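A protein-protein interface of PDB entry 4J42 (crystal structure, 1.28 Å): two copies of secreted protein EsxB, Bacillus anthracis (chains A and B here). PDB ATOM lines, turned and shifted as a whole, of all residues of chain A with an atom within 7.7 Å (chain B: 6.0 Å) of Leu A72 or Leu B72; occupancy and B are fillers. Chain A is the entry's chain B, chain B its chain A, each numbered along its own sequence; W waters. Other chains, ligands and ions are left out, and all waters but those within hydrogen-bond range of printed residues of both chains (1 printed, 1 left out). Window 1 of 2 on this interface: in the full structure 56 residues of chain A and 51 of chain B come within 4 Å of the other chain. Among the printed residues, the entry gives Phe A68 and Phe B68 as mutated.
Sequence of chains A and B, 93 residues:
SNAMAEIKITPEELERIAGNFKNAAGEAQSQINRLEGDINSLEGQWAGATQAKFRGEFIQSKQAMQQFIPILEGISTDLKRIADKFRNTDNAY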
ATOM      1  N   ASN A  20      14.173  29.213   9.965  1.00  0.00           N
ATOM      2  CA  ASN A  20      14.544  28.318   8.871  1.00  0.00           C
ATOM      3  C   ASN A  20      15.564  27.286   9.325  1.00  0.00           C
ATOM      4  O   ASN A  20      15.517  26.133   8.901  1.00  0.00           O
ATOM      5  CB  ASN A  20      15.049  29.098   7.658  1.00  0.00           C
ATOM      6  CG  ASN A  20      13.933  29.815   6.925  1.00  0.00           C
ATOM      7  OD1 ASN A  20      12.820  29.301   6.807  1.00  0.00           O
ATOM      8  ND2 ASN A  20      14.233  31.000   6.412  1.00  0.00           N
ATOM      9  N   PHE A  21      16.469  27.693  10.204  1.00  0.00           N
ATOM     10  CA  PHE A  21      17.484  26.787  10.726  1.00  0.00           C
ATOM     11  C   PHE A  21      16.869  25.766  11.689  1.00  0.00           C
ATOM     12  O   PHE A  21      17.177  24.575  11.610  1.00  0.00           O
ATOM     13  CB  PHE A  21      18.573  27.623  11.401  1.00  0.00           C
ATOM     14  CG  PHE A  21      19.850  26.888  11.668  1.00  0.00           C
ATOM     15  CD1 PHE A  21      20.151  25.679  11.046  1.00  0.00           C
ATOM     16  CD2 PHE A  21      20.776  27.437  12.544  1.00  0.00           C
ATOM     17  CE1 PHE A  21      21.352  25.032  11.319  1.00  0.00           C
ATOM     18  CE2 PHE A  21      21.966  26.801  12.813  1.00  0.00           C
ATOM     19  CZ  PHE A  21      22.254  25.600  12.213  1.00  0.00           C
ATOM     20  N   LYS A  22      15.992  26.217  12.584  1.00  0.00           N
ATOM     21  CA  LYS A  22      15.246  25.285  13.435  1.00  0.00           C
ATOM     22  C   LYS A  22      14.560  24.233  12.587  1.00  0.00           C
ATOM     23  O   LYS A  22      14.599  23.044  12.908  1.00  0.00           O
ATOM     24  CB  LYS A  22      14.191  26.009  14.270  1.00  0.00           C
ATOM     25  CG  LYS A  22      14.773  26.874  15.387  1.00  0.00           C
ATOM     26  CD  LYS A  22      13.678  27.431  16.265  1.00  0.00           C
ATOM     27  CE  LYS A  22      14.221  28.405  17.300  1.00  0.00           C
ATOM     28  NZ  LYS A  22      13.230  28.751  18.372  1.00  0.00           N
ATOM     29  N   ASN A  23      13.928  24.672  11.501  1.00  0.00           N
ATOM     30  CA  ASN A  23      13.206  23.751  10.628  1.00  0.00           C
ATOM     31  C   ASN A  23      14.145  22.761   9.951  1.00  0.00           C
ATOM     32  O   ASN A  23      13.830  21.568   9.855  1.00  0.00           O
ATOM     33  CB  ASN A  23      12.398  24.511   9.575  1.00  0.00           C
ATOM     34  CG  ASN A  23      11.188  25.214  10.161  1.00  0.00           C
ATOM     35  OD1 ASN A  23      10.753  24.900  11.275  1.00  0.00           O
ATOM     36  ND2 ASN A  23      10.626  26.154   9.406  1.00  0.00           N
ATOM     37  N   ALA A  24      15.291  23.240   9.475  1.00  0.00           N
ATOM     38  CA  ALA A  24      16.255  22.347   8.835  1.00  0.00           C
ATOM     39  C   ALA A  24      16.746  21.282   9.811  1.00  0.00           C
ATOM     40  O   ALA A  24      16.892  20.111   9.444  1.00  0.00           O
ATOM     41  CB  ALA A  24      17.414  23.140   8.268  1.00  0.00           C
ATOM     42  N   ALA A  25      17.002  21.677  11.050  1.00  0.00           N
ATOM     43  CA  ALA A  25      17.447  20.739  12.068  1.00  0.00           C
ATOM     44  C   ALA A  25      16.334  19.786  12.479  1.00  0.00           C
ATOM     45  O   ALA A  25      16.571  18.585  12.685  1.00  0.00           O
ATOM     46  CB  ALA A  25      17.968  21.489  13.272  1.00  0.00           C
ATOM     47  N   GLY A  26      15.116  20.303  12.608  1.00  0.00           N
ATOM     48  CA  GLY A  26      13.963  19.487  12.954  1.00  0.00           C
ATOM     49  C   GLY A  26      13.671  18.431  11.911  1.00  0.00           C
ATOM     50  O   GLY A  26      13.311  17.297  12.251  1.00  0.00           O
ATOM     51  N   GLU A  27      13.837  18.783  10.640  1.00  0.00           N
ATOM     52  CA  GLU A  27      13.660  17.835   9.541  1.00  0.00           C
ATOM     53  C   GLU A  27      14.693  16.712   9.591  1.00  0.00           C
ATOM     54  O   GLU A  27      14.374  15.550   9.287  1.00  0.00           O
ATOM     55  CB  GLU A  27      13.725  18.554   8.191  1.00  0.00           C
ATOM     56  CG  GLU A  27      12.520  19.447   7.907  1.00  0.00           C
ATOM     57  CD  GLU A  27      12.787  20.513   6.842  1.00  0.00           C
ATOM     58  OE1 GLU A  27      13.938  20.647   6.358  1.00  0.00           O
ATOM     59  OE2 GLU A  27      11.833  21.235   6.485  1.00  0.00           O
ATOM     60  N   ALA A  28      15.927  17.042   9.951  1.00  0.00           N
ATOM     61  CA  ALA A  28      16.950  16.009  10.119  1.00  0.00           C
ATOM     62  C   ALA A  28      16.581  15.072  11.265  1.00  0.00           C
ATOM     63  O   ALA A  28      16.727  13.854  11.143  1.00  0.00           O
ATOM     64  CB  ALA A  28      18.313  16.629  10.345  1.00  0.00           C
ATOM     65  N   GLN A  29      16.093  15.622  12.371  1.00  0.00           N
ATOM     66  CA  GLN A  29      15.633  14.806  13.490  1.00  0.00           C
ATOM     67  C   GLN A  29      14.478  13.902  13.062  1.00  0.00           C
ATOM     68  O   GLN A  29      14.420  12.725  13.442  1.00  0.00           O
ATOM     69  CB  GLN A  29      15.211  15.708  14.652  1.00  0.00           C
ATOM     70  CG  GLN A  29      14.914  14.993  15.969  1.00  0.00           C
ATOM     71  CD  GLN A  29      16.142  14.362  16.617  1.00  0.00           C
ATOM     72  OE1 GLN A  29      16.224  13.132  16.730  1.00  0.00           O
ATOM     73  NE2 GLN A  29      17.092  15.198  17.069  1.00  0.00           N
ATOM     74  N   ALA A  64      26.190   6.828   6.579  1.00  0.00           N
ATOM     75  CA  ALA A  64      25.468   8.100   6.620  1.00  0.00           C
ATOM     76  C   ALA A  64      25.373   8.628   8.046  1.00  0.00           C
ATOM     77  O   ALA A  64      25.701   9.796   8.317  1.00  0.00           O
ATOM     78  CB  ALA A  64      24.071   7.930   6.042  1.00  0.00           C
ATOM     79  N   MET A  65      24.922   7.782   8.965  1.00  0.00           N
ATOM     80  CA  MET A  65      24.711   8.225  10.334  1.00  0.00           C
ATOM     81  C   MET A  65      26.031   8.592  11.002  1.00  0.00           C
ATOM     82  O   MET A  65      26.152   9.659  11.616  1.00  0.00           O
ATOM     83  CB  MET A  65      23.960   7.164  11.137  1.00  0.00           C
ATOM     84  CG  MET A  65      22.565   6.886  10.622  1.00  0.00           C
ATOM     85  SD  MET A  65      21.648   5.737  11.691  1.00  0.00           S
ATOM     86  CE  MET A  65      22.495   4.193  11.390  1.00  0.00           C
ATOM     87  N   GLN A  67      28.993   9.373   9.663  1.00  0.00           N
ATOM     88  CA  GLN A  67      29.794  10.430   9.068  1.00  0.00           C
ATOM     89  C   GLN A  67      29.277  11.812   9.450  1.00  0.00           C
ATOM     90  O   GLN A  67      30.048  12.777   9.528  1.00  0.00           O
ATOM     91  CB  GLN A  67      29.872  10.289   7.546  1.00  0.00           C
ATOM     92  CG  GLN A  67      28.625  10.743   6.797  1.00  0.00           C
ATOM     93  CD  GLN A  67      28.632  10.326   5.334  1.00  0.00           C
ATOM     94  OE1 GLN A  67      29.461   9.526   4.903  1.00  0.00           O
ATOM     95  NE2 GLN A  67      27.700  10.871   4.558  1.00  0.00           N
ATOM     96  N   PHE A  68      27.977  11.925   9.686  1.00  0.00           N
ATOM     97  CA  PHE A  68      27.407  13.229   9.985  1.00  0.00           C
ATOM     98  C   PHE A  68      27.537  13.631  11.443  1.00  0.00           C
ATOM     99  O   PHE A  68      27.382  14.820  11.763  1.00  0.00           O
ATOM    100  CB  PHE A  68      25.950  13.304   9.553  1.00  0.00           C
ATOM    101  CG  PHE A  68      25.747  13.353   8.061  1.00  0.00           C
ATOM    102  CD1 PHE A  68      26.496  14.191   7.255  1.00  0.00           C
ATOM    103  CD2 PHE A  68      24.762  12.574   7.470  1.00  0.00           C
ATOM    104  CE1 PHE A  68      26.266  14.231   5.867  1.00  0.00           C
ATOM    105  CE2 PHE A  68      24.537  12.614   6.099  1.00  0.00           C
ATOM    106  CZ  PHE A  68      25.286  13.435   5.308  1.00  0.00           C
ATOM    107  N   ILE A  69      27.822  12.689  12.332  1.00  0.00           N
ATOM    108  CA  ILE A  69      27.952  13.035  13.745  1.00  0.00           C
ATOM    109  C   ILE A  69      29.016  14.128  14.001  1.00  0.00           C
ATOM    110  O   ILE A  69      28.704  15.134  14.638  1.00  0.00           O
ATOM    111  CB  ILE A  69      28.134  11.777  14.625  1.00  0.00           C
ATOM    112  CG1 ILE A  69      26.806  11.009  14.701  1.00  0.00           C
ATOM    113  CG2 ILE A  69      28.617  12.162  16.017  1.00  0.00           C
ATOM    114  CD1 ILE A  69      26.919   9.581  15.209  1.00  0.00           C
ATOM    115  N   PRO A  70      30.254  13.977  13.482  1.00  0.00           N
ATOM    116  CA  PRO A  70      31.223  15.052  13.768  1.00  0.00           C
ATOM    117  C   PRO A  70      30.887  16.365  13.069  1.00  0.00           C
ATOM    118  O   PRO A  70      31.289  17.438  13.534  1.00  0.00           O
ATOM    119  CB  PRO A  70      32.552  14.492  13.248  1.00  0.00           C
ATOM    120  CG  PRO A  70      32.163  13.398  12.296  1.00  0.00           C
ATOM    121  CD  PRO A  70      30.888  12.813  12.833  1.00  0.00           C
ATOM    122  N   ILE A  71      30.151  16.304  11.971  1.00  0.00           N
ATOM    123  CA  ILE A  71      29.729  17.521  11.294  1.00  0.00           C
ATOM    124  C   ILE A  71      28.685  18.263  12.138  1.00  0.00           C
ATOM    125  O   ILE A  71      28.779  19.482  12.340  1.00  0.00           O
ATOM    126  CB  ILE A  71      29.234  17.212   9.866  1.00  0.00           C
ATOM    127  CG1 ILE A  71      30.429  16.741   9.017  1.00  0.00           C
ATOM    128  CG2 ILE A  71      28.555  18.420   9.238  1.00  0.00           C
ATOM    129  CD1 ILE A  71      30.073  16.076   7.692  1.00  0.00           C
ATOM    130  N   LEU A  72      27.708  17.529  12.657  1.00  0.00           N
ATOM    131  CA  LEU A  72      26.717  18.098  13.559  1.00  0.00           C
ATOM    132  C   LEU A  72      27.370  18.636  14.826  1.00  0.00           C
ATOM    133  O   LEU A  72      26.975  19.690  15.319  1.00  0.00           O
ATOM    134  CB  LEU A  72      25.657  17.050  13.911  1.00  0.00           C
ATOM    135  CG  LEU A  72      24.736  16.678  12.749  1.00  0.00           C
ATOM    136  CD1 LEU A  72      23.962  15.423  13.087  1.00  0.00           C
ATOM    137  CD2 LEU A  72      23.785  17.832  12.416  1.00  0.00           C
ATOM    138  N   GLU A  73      28.358  17.927  15.355  1.00  0.00           N
ATOM    139  CA  GLU A  73      29.086  18.385  16.535  1.00  0.00           C
ATOM    140  C   GLU A  73      29.852  19.678  16.257  1.00  0.00           C
ATOM    141  O   GLU A  73      29.936  20.552  17.127  1.00  0.00           O
ATOM    142  CB  GLU A  73      30.021  17.287  17.044  1.00  0.00           C
ATOM    143  CG  GLU A  73      29.270  16.128  17.695  1.00  0.00           C
ATOM    144  CD  GLU A  73      30.135  14.916  17.976  1.00  0.00           C
ATOM    145  OE1 GLU A  73      31.205  14.768  17.345  1.00  0.00           O
ATOM    146  OE2 GLU A  73      29.728  14.085  18.821  1.00  0.00           O
ATOM    147  N   GLY A  74      30.403  19.810  15.052  1.00  0.00           N
ATOM    148  CA  GLY A  74      31.092  21.031  14.661  1.00  0.00           C
ATOM    149  C   GLY A  74      30.107  22.184  14.620  1.00  0.00           C
ATOM    150  O   GLY A  74      30.382  23.282  15.125  1.00  0.00           O
ATOM    151  N   ILE A  75      28.941  21.943  14.037  1.00  0.00           N
ATOM    152  CA  ILE A  75      27.883  22.945  13.978  1.00  0.00           C
ATOM    153  C   ILE A  75      27.420  23.347  15.373  1.00  0.00           C
ATOM    154  O   ILE A  75      27.326  24.538  15.686  1.00  0.00           O
ATOM    155  CB  ILE A  75      26.699  22.447  13.125  1.00  0.00           C
ATOM    156  CG1 ILE A  75      27.107  22.431  11.651  1.00  0.00           C
ATOM    157  CG2 ILE A  75      25.438  23.268  13.373  1.00  0.00           C
ATOM    158  CD1 ILE A  75      26.106  21.743  10.731  1.00  0.00           C
ATOM    159  N   SER A  76      27.164  22.371  16.234  1.00  0.00           N
ATOM    160  CA  SER A  76      26.663  22.681  17.572  1.00  0.00           C
ATOM    161  C   SER A  76      27.713  23.445  18.384  1.00  0.00           C
ATOM    162  O   SER A  76      27.389  24.429  19.056  1.00  0.00           O
ATOM    163  CB  SER A  76      26.147  21.415  18.279  1.00  0.00           C
ATOM    164  OG  SER A  76      27.186  20.515  18.571  1.00  0.00           O
ATOM    165  N   THR A  77      28.972  23.035  18.293  1.00  0.00           N
ATOM    166  CA  THR A  77      30.042  23.768  18.965  1.00  0.00           C
ATOM    167  C   THR A  77      30.186  25.203  18.438  1.00  0.00           C
ATOM    168  O   THR A  77      30.378  26.150  19.210  1.00  0.00           O
ATOM    169  CB  THR A  77      31.382  23.034  18.842  1.00  0.00           C
ATOM    170  OG1 THR A  77      31.272  21.748  19.464  1.00  0.00           O
ATOM    171  CG2 THR A  77      32.494  23.819  19.529  1.00  0.00           C
ATOM    172  N   ASP A  78      30.091  25.363  17.122  1.00  0.00           N
ATOM    173  CA  ASP A  78      30.177  26.684  16.508  1.00  0.00           C
ATOM    174  C   ASP A  78      29.083  27.599  17.056  1.00  0.00           C
ATOM    175  O   ASP A  78      29.331  28.759  17.374  1.00  0.00           O
ATOM    176  CB  ASP A  78      30.011  26.600  14.986  1.00  0.00           C
ATOM    177  CG  ASP A  78      31.222  26.034  14.271  1.00  0.00           C
ATOM    178  OD1 ASP A  78      32.338  26.011  14.821  1.00  0.00           O
ATOM    179  OD2 ASP A  78      31.018  25.615  13.098  1.00  0.00           O
ATOM    180  N   LEU A  79      27.862  27.075  17.149  1.00  0.00           N
ATOM    181  CA  LEU A  79      26.739  27.858  17.649  1.00  0.00           C
ATOM    182  C   LEU A  79      26.880  28.161  19.132  1.00  0.00           C
ATOM    183  O   LEU A  79      26.579  29.261  19.579  1.00  0.00           O
ATOM    184  CB  LEU A  79      25.416  27.138  17.374  1.00  0.00           C
ATOM    185  CG  LEU A  79      25.092  26.927  15.894  1.00  0.00           C
ATOM    186  CD1 LEU A  79      23.857  26.044  15.768  1.00  0.00           C
ATOM    187  CD2 LEU A  79      24.901  28.251  15.174  1.00  0.00           C
ATOM    188  N   PHE B  21      23.320   9.681  16.533  1.00  0.00           N
ATOM    189  CA  PHE B  21      22.934  10.726  15.588  1.00  0.00           C
ATOM    190  C   PHE B  21      21.819  11.601  16.169  1.00  0.00           C
ATOM    191  O   PHE B  21      21.890  12.824  16.077  1.00  0.00           O
ATOM    192  CB  PHE B  21      22.533  10.137  14.218  1.00  0.00           C
ATOM    193  CG  PHE B  21      22.147  11.185  13.195  1.00  0.00           C
ATOM    194  CD1 PHE B  21      20.922  11.835  13.286  1.00  0.00           C
ATOM    195  CD2 PHE B  21      23.005  11.539  12.163  1.00  0.00           C
ATOM    196  CE1 PHE B  21      20.548  12.809  12.378  1.00  0.00           C
ATOM    197  CE2 PHE B  21      22.619  12.509  11.240  1.00  0.00           C
ATOM    198  CZ  PHE B  21      21.391  13.145  11.363  1.00  0.00           C
ATOM    199  N   ALA B  24      23.438  13.988  18.498  1.00  0.00           N
ATOM    200  CA  ALA B  24      24.198  15.039  17.834  1.00  0.00           C
ATOM    201  C   ALA B  24      23.263  16.079  17.191  1.00  0.00           C
ATOM    202  O   ALA B  24      23.517  17.298  17.272  1.00  0.00           O
ATOM    203  CB  ALA B  24      25.156  14.436  16.815  1.00  0.00           C
ATOM    204  N   ALA B  25      22.187  15.617  16.561  1.00  0.00           N
ATOM    205  CA  ALA B  25      21.211  16.526  15.949  1.00  0.00           C
ATOM    206  C   ALA B  25      20.475  17.320  17.023  1.00  0.00           C
ATOM    207  O   ALA B  25      20.226  18.524  16.862  1.00  0.00           O
ATOM    208  CB  ALA B  25      20.228  15.758  15.091  1.00  0.00           C
ATOM    209  N   ALA B  28      22.523  20.169  18.284  1.00  0.00           N
ATOM    210  CA  ALA B  28      22.429  21.284  17.348  1.00  0.00           C
ATOM    211  C   ALA B  28      21.113  22.034  17.541  1.00  0.00           C
ATOM    212  O   ALA B  28      21.104  23.266  17.597  1.00  0.00           O
ATOM    213  CB  ALA B  28      22.587  20.809  15.909  1.00  0.00           C
ATOM    214  N   PHE B  68      24.745  27.064   7.712  1.00  0.00           N
ATOM    215  CA  PHE B  68      24.472  25.734   8.239  1.00  0.00           C
ATOM    216  C   PHE B  68      23.119  25.186   7.793  1.00  0.00           C
ATOM    217  O   PHE B  68      22.931  23.963   7.759  1.00  0.00           O
ATOM    218  CB  PHE B  68      24.558  25.726   9.759  1.00  0.00           C
ATOM    219  CG  PHE B  68      25.923  26.051  10.310  1.00  0.00           C
ATOM    220  CD1 PHE B  68      27.068  25.946   9.544  1.00  0.00           C
ATOM    221  CD2 PHE B  68      26.045  26.450  11.637  1.00  0.00           C
ATOM    222  CE1 PHE B  68      28.315  26.249  10.094  1.00  0.00           C
ATOM    223  CE2 PHE B  68      27.276  26.748  12.183  1.00  0.00           C
ATOM    224  CZ  PHE B  68      28.405  26.647  11.416  1.00  0.00           C
ATOM    225  N   ILE B  69      22.182  26.059   7.442  1.00  0.00           N
ATOM    226  CA  ILE B  69      20.895  25.613   6.908  1.00  0.00           C
ATOM    227  C   ILE B  69      21.048  24.585   5.766  1.00  0.00           C
ATOM    228  O   ILE B  69      20.469  23.494   5.848  1.00  0.00           O
ATOM    229  CB  ILE B  69      19.997  26.808   6.487  1.00  0.00           C
ATOM    230  CG1 ILE B  69      19.472  27.540   7.726  1.00  0.00           C
ATOM    231  CG2 ILE B  69      18.855  26.335   5.585  1.00  0.00           C
ATOM    232  CD1 ILE B  69      18.909  28.933   7.432  1.00  0.00           C
ATOM    233  N   PRO B  70      21.823  24.903   4.709  1.00  0.00           N
ATOM    234  CA  PRO B  70      21.908  23.930   3.609  1.00  0.00           C
ATOM    235  C   PRO B  70      22.643  22.649   3.992  1.00  0.00           C
ATOM    236  O   PRO B  70      22.394  21.594   3.393  1.00  0.00           O
ATOM    237  CB  PRO B  70      22.663  24.694   2.504  1.00  0.00           C
ATOM    238  CG  PRO B  70      23.371  25.819   3.225  1.00  0.00           C
ATOM    239  CD  PRO B  70      22.476  26.182   4.361  1.00  0.00           C
ATOM    240  N   ILE B  71      23.537  22.710   4.971  1.00  0.00           N
ATOM    241  CA  ILE B  71      24.192  21.484   5.421  1.00  0.00           C
ATOM    242  C   ILE B  71      23.161  20.555   6.061  1.00  0.00           C
ATOM    243  O   ILE B  71      23.102  19.364   5.756  1.00  0.00           O
ATOM    244  CB  ILE B  71      25.375  21.765   6.382  1.00  0.00           C
ATOM    245  CG1 ILE B  71      26.432  22.616   5.671  1.00  0.00           C
ATOM    246  CG2 ILE B  71      25.962  20.453   6.907  1.00  0.00           C
ATOM    247  CD1 ILE B  71      27.611  23.001   6.553  1.00  0.00           C
ATOM    248  N   LEU B  72      22.323  21.092   6.934  1.00  0.00           N
ATOM    249  CA  LEU B  72      21.271  20.296   7.551  1.00  0.00           C
ATOM    250  C   LEU B  72      20.279  19.784   6.525  1.00  0.00           C
ATOM    251  O   LEU B  72      19.810  18.651   6.632  1.00  0.00           O
ATOM    252  CB  LEU B  72      20.560  21.092   8.645  1.00  0.00           C
ATOM    253  CG  LEU B  72      21.142  20.940  10.048  1.00  0.00           C
ATOM    254  CD1 LEU B  72      20.919  19.512  10.540  1.00  0.00           C
ATOM    255  CD2 LEU B  72      22.598  21.296  10.121  1.00  0.00           C
ATOM    256  N   GLU B  73      19.961  20.594   5.524  1.00  0.00           N
ATOM    257  CA  GLU B  73      19.052  20.157   4.477  1.00  0.00           C
ATOM    258  C   GLU B  73      19.640  18.993   3.683  1.00  0.00           C
ATOM    259  O   GLU B  73      18.915  18.068   3.305  1.00  0.00           O
ATOM    260  CB  GLU B  73      18.695  21.318   3.544  1.00  0.00           C
ATOM    261  CG  GLU B  73      17.832  22.368   4.215  1.00  0.00           C
ATOM    262  CD  GLU B  73      17.623  23.604   3.358  1.00  0.00           C
ATOM    263  OE1 GLU B  73      18.502  23.917   2.525  1.00  0.00           O
ATOM    264  OE2 GLU B  73      16.580  24.272   3.527  1.00  0.00           O
ATOM    265  N   GLY B  74      20.943  19.023   3.418  1.00  0.00           N
ATOM    266  CA  GLY B  74      21.584  17.919   2.725  1.00  0.00           C
ATOM    267  C   GLY B  74      21.527  16.651   3.562  1.00  0.00           C
ATOM    268  O   GLY B  74      21.293  15.548   3.044  1.00  0.00           O
ATOM    269  N   ILE B  75      21.730  16.792   4.866  1.00  0.00           N
ATOM    270  CA  ILE B  75      21.675  15.652   5.773  1.00  0.00           C
ATOM    271  C   ILE B  75      20.281  15.047   5.791  1.00  0.00           C
ATOM    272  O   ILE B  75      20.120  13.829   5.644  1.00  0.00           O
ATOM    273  CB  ILE B  75      22.120  16.056   7.195  1.00  0.00           C
ATOM    274  CG1 ILE B  75      23.622  16.352   7.197  1.00  0.00           C
ATOM    275  CG2 ILE B  75      21.764  14.967   8.204  1.00  0.00           C
ATOM    276  CD1 ILE B  75      24.130  17.000   8.473  1.00  0.00           C
ATOM    277  N   SER B  76      19.259  15.882   5.950  1.00  0.00           N
ATOM    278  CA  SER B  76      17.905  15.354   6.029  1.00  0.00           C
ATOM    279  C   SER B  76      17.477  14.710   4.713  1.00  0.00           C
ATOM    280  O   SER B  76      16.808  13.684   4.723  1.00  0.00           O
ATOM    281  CB  SER B  76      16.920  16.431   6.491  1.00  0.00           C
ATOM    282  OG  SER B  76      16.718  17.394   5.481  1.00  0.00           O
ATOM    283  N   THR B  77      17.897  15.278   3.589  1.00  0.00           N
ATOM    284  CA  THR B  77      17.540  14.719   2.288  1.00  0.00           C
ATOM    285  C   THR B  77      18.178  13.342   2.098  1.00  0.00           C
ATOM    286  O   THR B  77      17.547  12.414   1.595  1.00  0.00           O
ATOM    287  CB  THR B  77      17.972  15.666   1.150  1.00  0.00           C
ATOM    288  OG1 THR B  77      17.237  16.895   1.251  1.00  0.00           O
ATOM    289  CG2 THR B  77      17.712  15.040  -0.208  1.00  0.00           C
HETATM  290  O   HOH W   1      26.112  17.993  18.049  1.00  0.00           O
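O of Glu B73 sits at hydrogen-bond distance from OG of Ser B76 (3.2 Å).
The backbone carbonyl oxygen (O) of Leu A72 sits at hydrogen-bond distance from the side-chain hydroxyl (OG) of Ser A76 (3.4 Å).
The side-chain hydroxyl (OG) of Ser A76 lies within hydrogen-bond range of the backbone carbonyl oxygen (O) of Glu A73, at 3.1 Å.
CB of Asn A20 touches CD1 of Ile B69, 3.9 Å away.
Ile B69 touches Ala A24.
Ala A24 touches Leu B72.
Leu B72 touches Ala A28.
Ser B76 touches Ala A28 (CB to N, 3.7 Å).
CD2 of Phe B21 touches O of Met A65, 3.7 Å away.
Phe B21 touches Ile A69 (N to CD1, 3.8 Å).
Leu A72 touches Ala B25 (CD1 to N, 3.9 Å).
CG2 of Ile A75 touches CD2 of Phe B68, at 3.7 Å.
CD2 of Leu B72 touches CD1 of Ile A75, 3.6 Å away.
Of the printed residues of chain B, Gln A29 touches Ala B25 (3.7 Å).
Of the printed residues of chain B, Phe A68 touches Phe B21 (3.8 Å) and Ile B75 (3.6 Å).
Leu A72 touches just these residues of chain B: Phe B21, Ala B24, Ala B25 and Leu B72.
Of the printed residues of chain B, Asp A78 touches Phe B68 (3.3 Å).
Of the printed residues of chain A, Leu B72 touches Ala A24 (3.8 Å), Ala A25 (3.99 Å), Ala A28 (3.9 Å), Leu A72 (3.8 Å) and Ile A75 (3.6 Å).
Printed residues of chain A within 4 Å of Ile B75: Phe A68 (3.6 Å).
Printed residues of chain A that touch a printed residue of chain B: Asn A20, Phe A21, Ala A24, Ala A25, Glu A27, Ala A28, Gln A29, Met A65, Phe A68, Ile A69, Leu A72, Ile A75, Ser A76 and Asp A78.
Hydrophobic or aromatic side chains of chain A that line the printed part of chain B: Phe A21, Ala A24, Ala A28, Phe A68, Ile A69, Leu A72 and Ile A75.
Of the 14 printed residues of chain B, 9 touch a printed residue of chain A.
Along chain B the printed residues that touch a printed residue of chain A span positions 21 to 76.
Phe A21 touches Phe B68, and with the chains exchanged Phe A68 touches Phe B21.
Phe A21 touches Ile B69, and with the chains exchanged Ile A69 touches Phe B21.
Phe A68 touches Ile B75, and with the chains exchanged Ile A75 touches Phe B68.
Leu A72 touches its own counterpart, Leu B72.
Of the 22 pairs that touch across the chains among the printed residues, 13 have their exchanged pair printed and touching as well.
Water W1 lies within hydrogen-bond range of the side-chain hydroxyl of Ser A76 (2.8 Å), the backbone carbonyl oxygen of Ala B24 (2.8 Å) and the backbone carbonyl oxygen of Leu A72 (3.3 Å).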
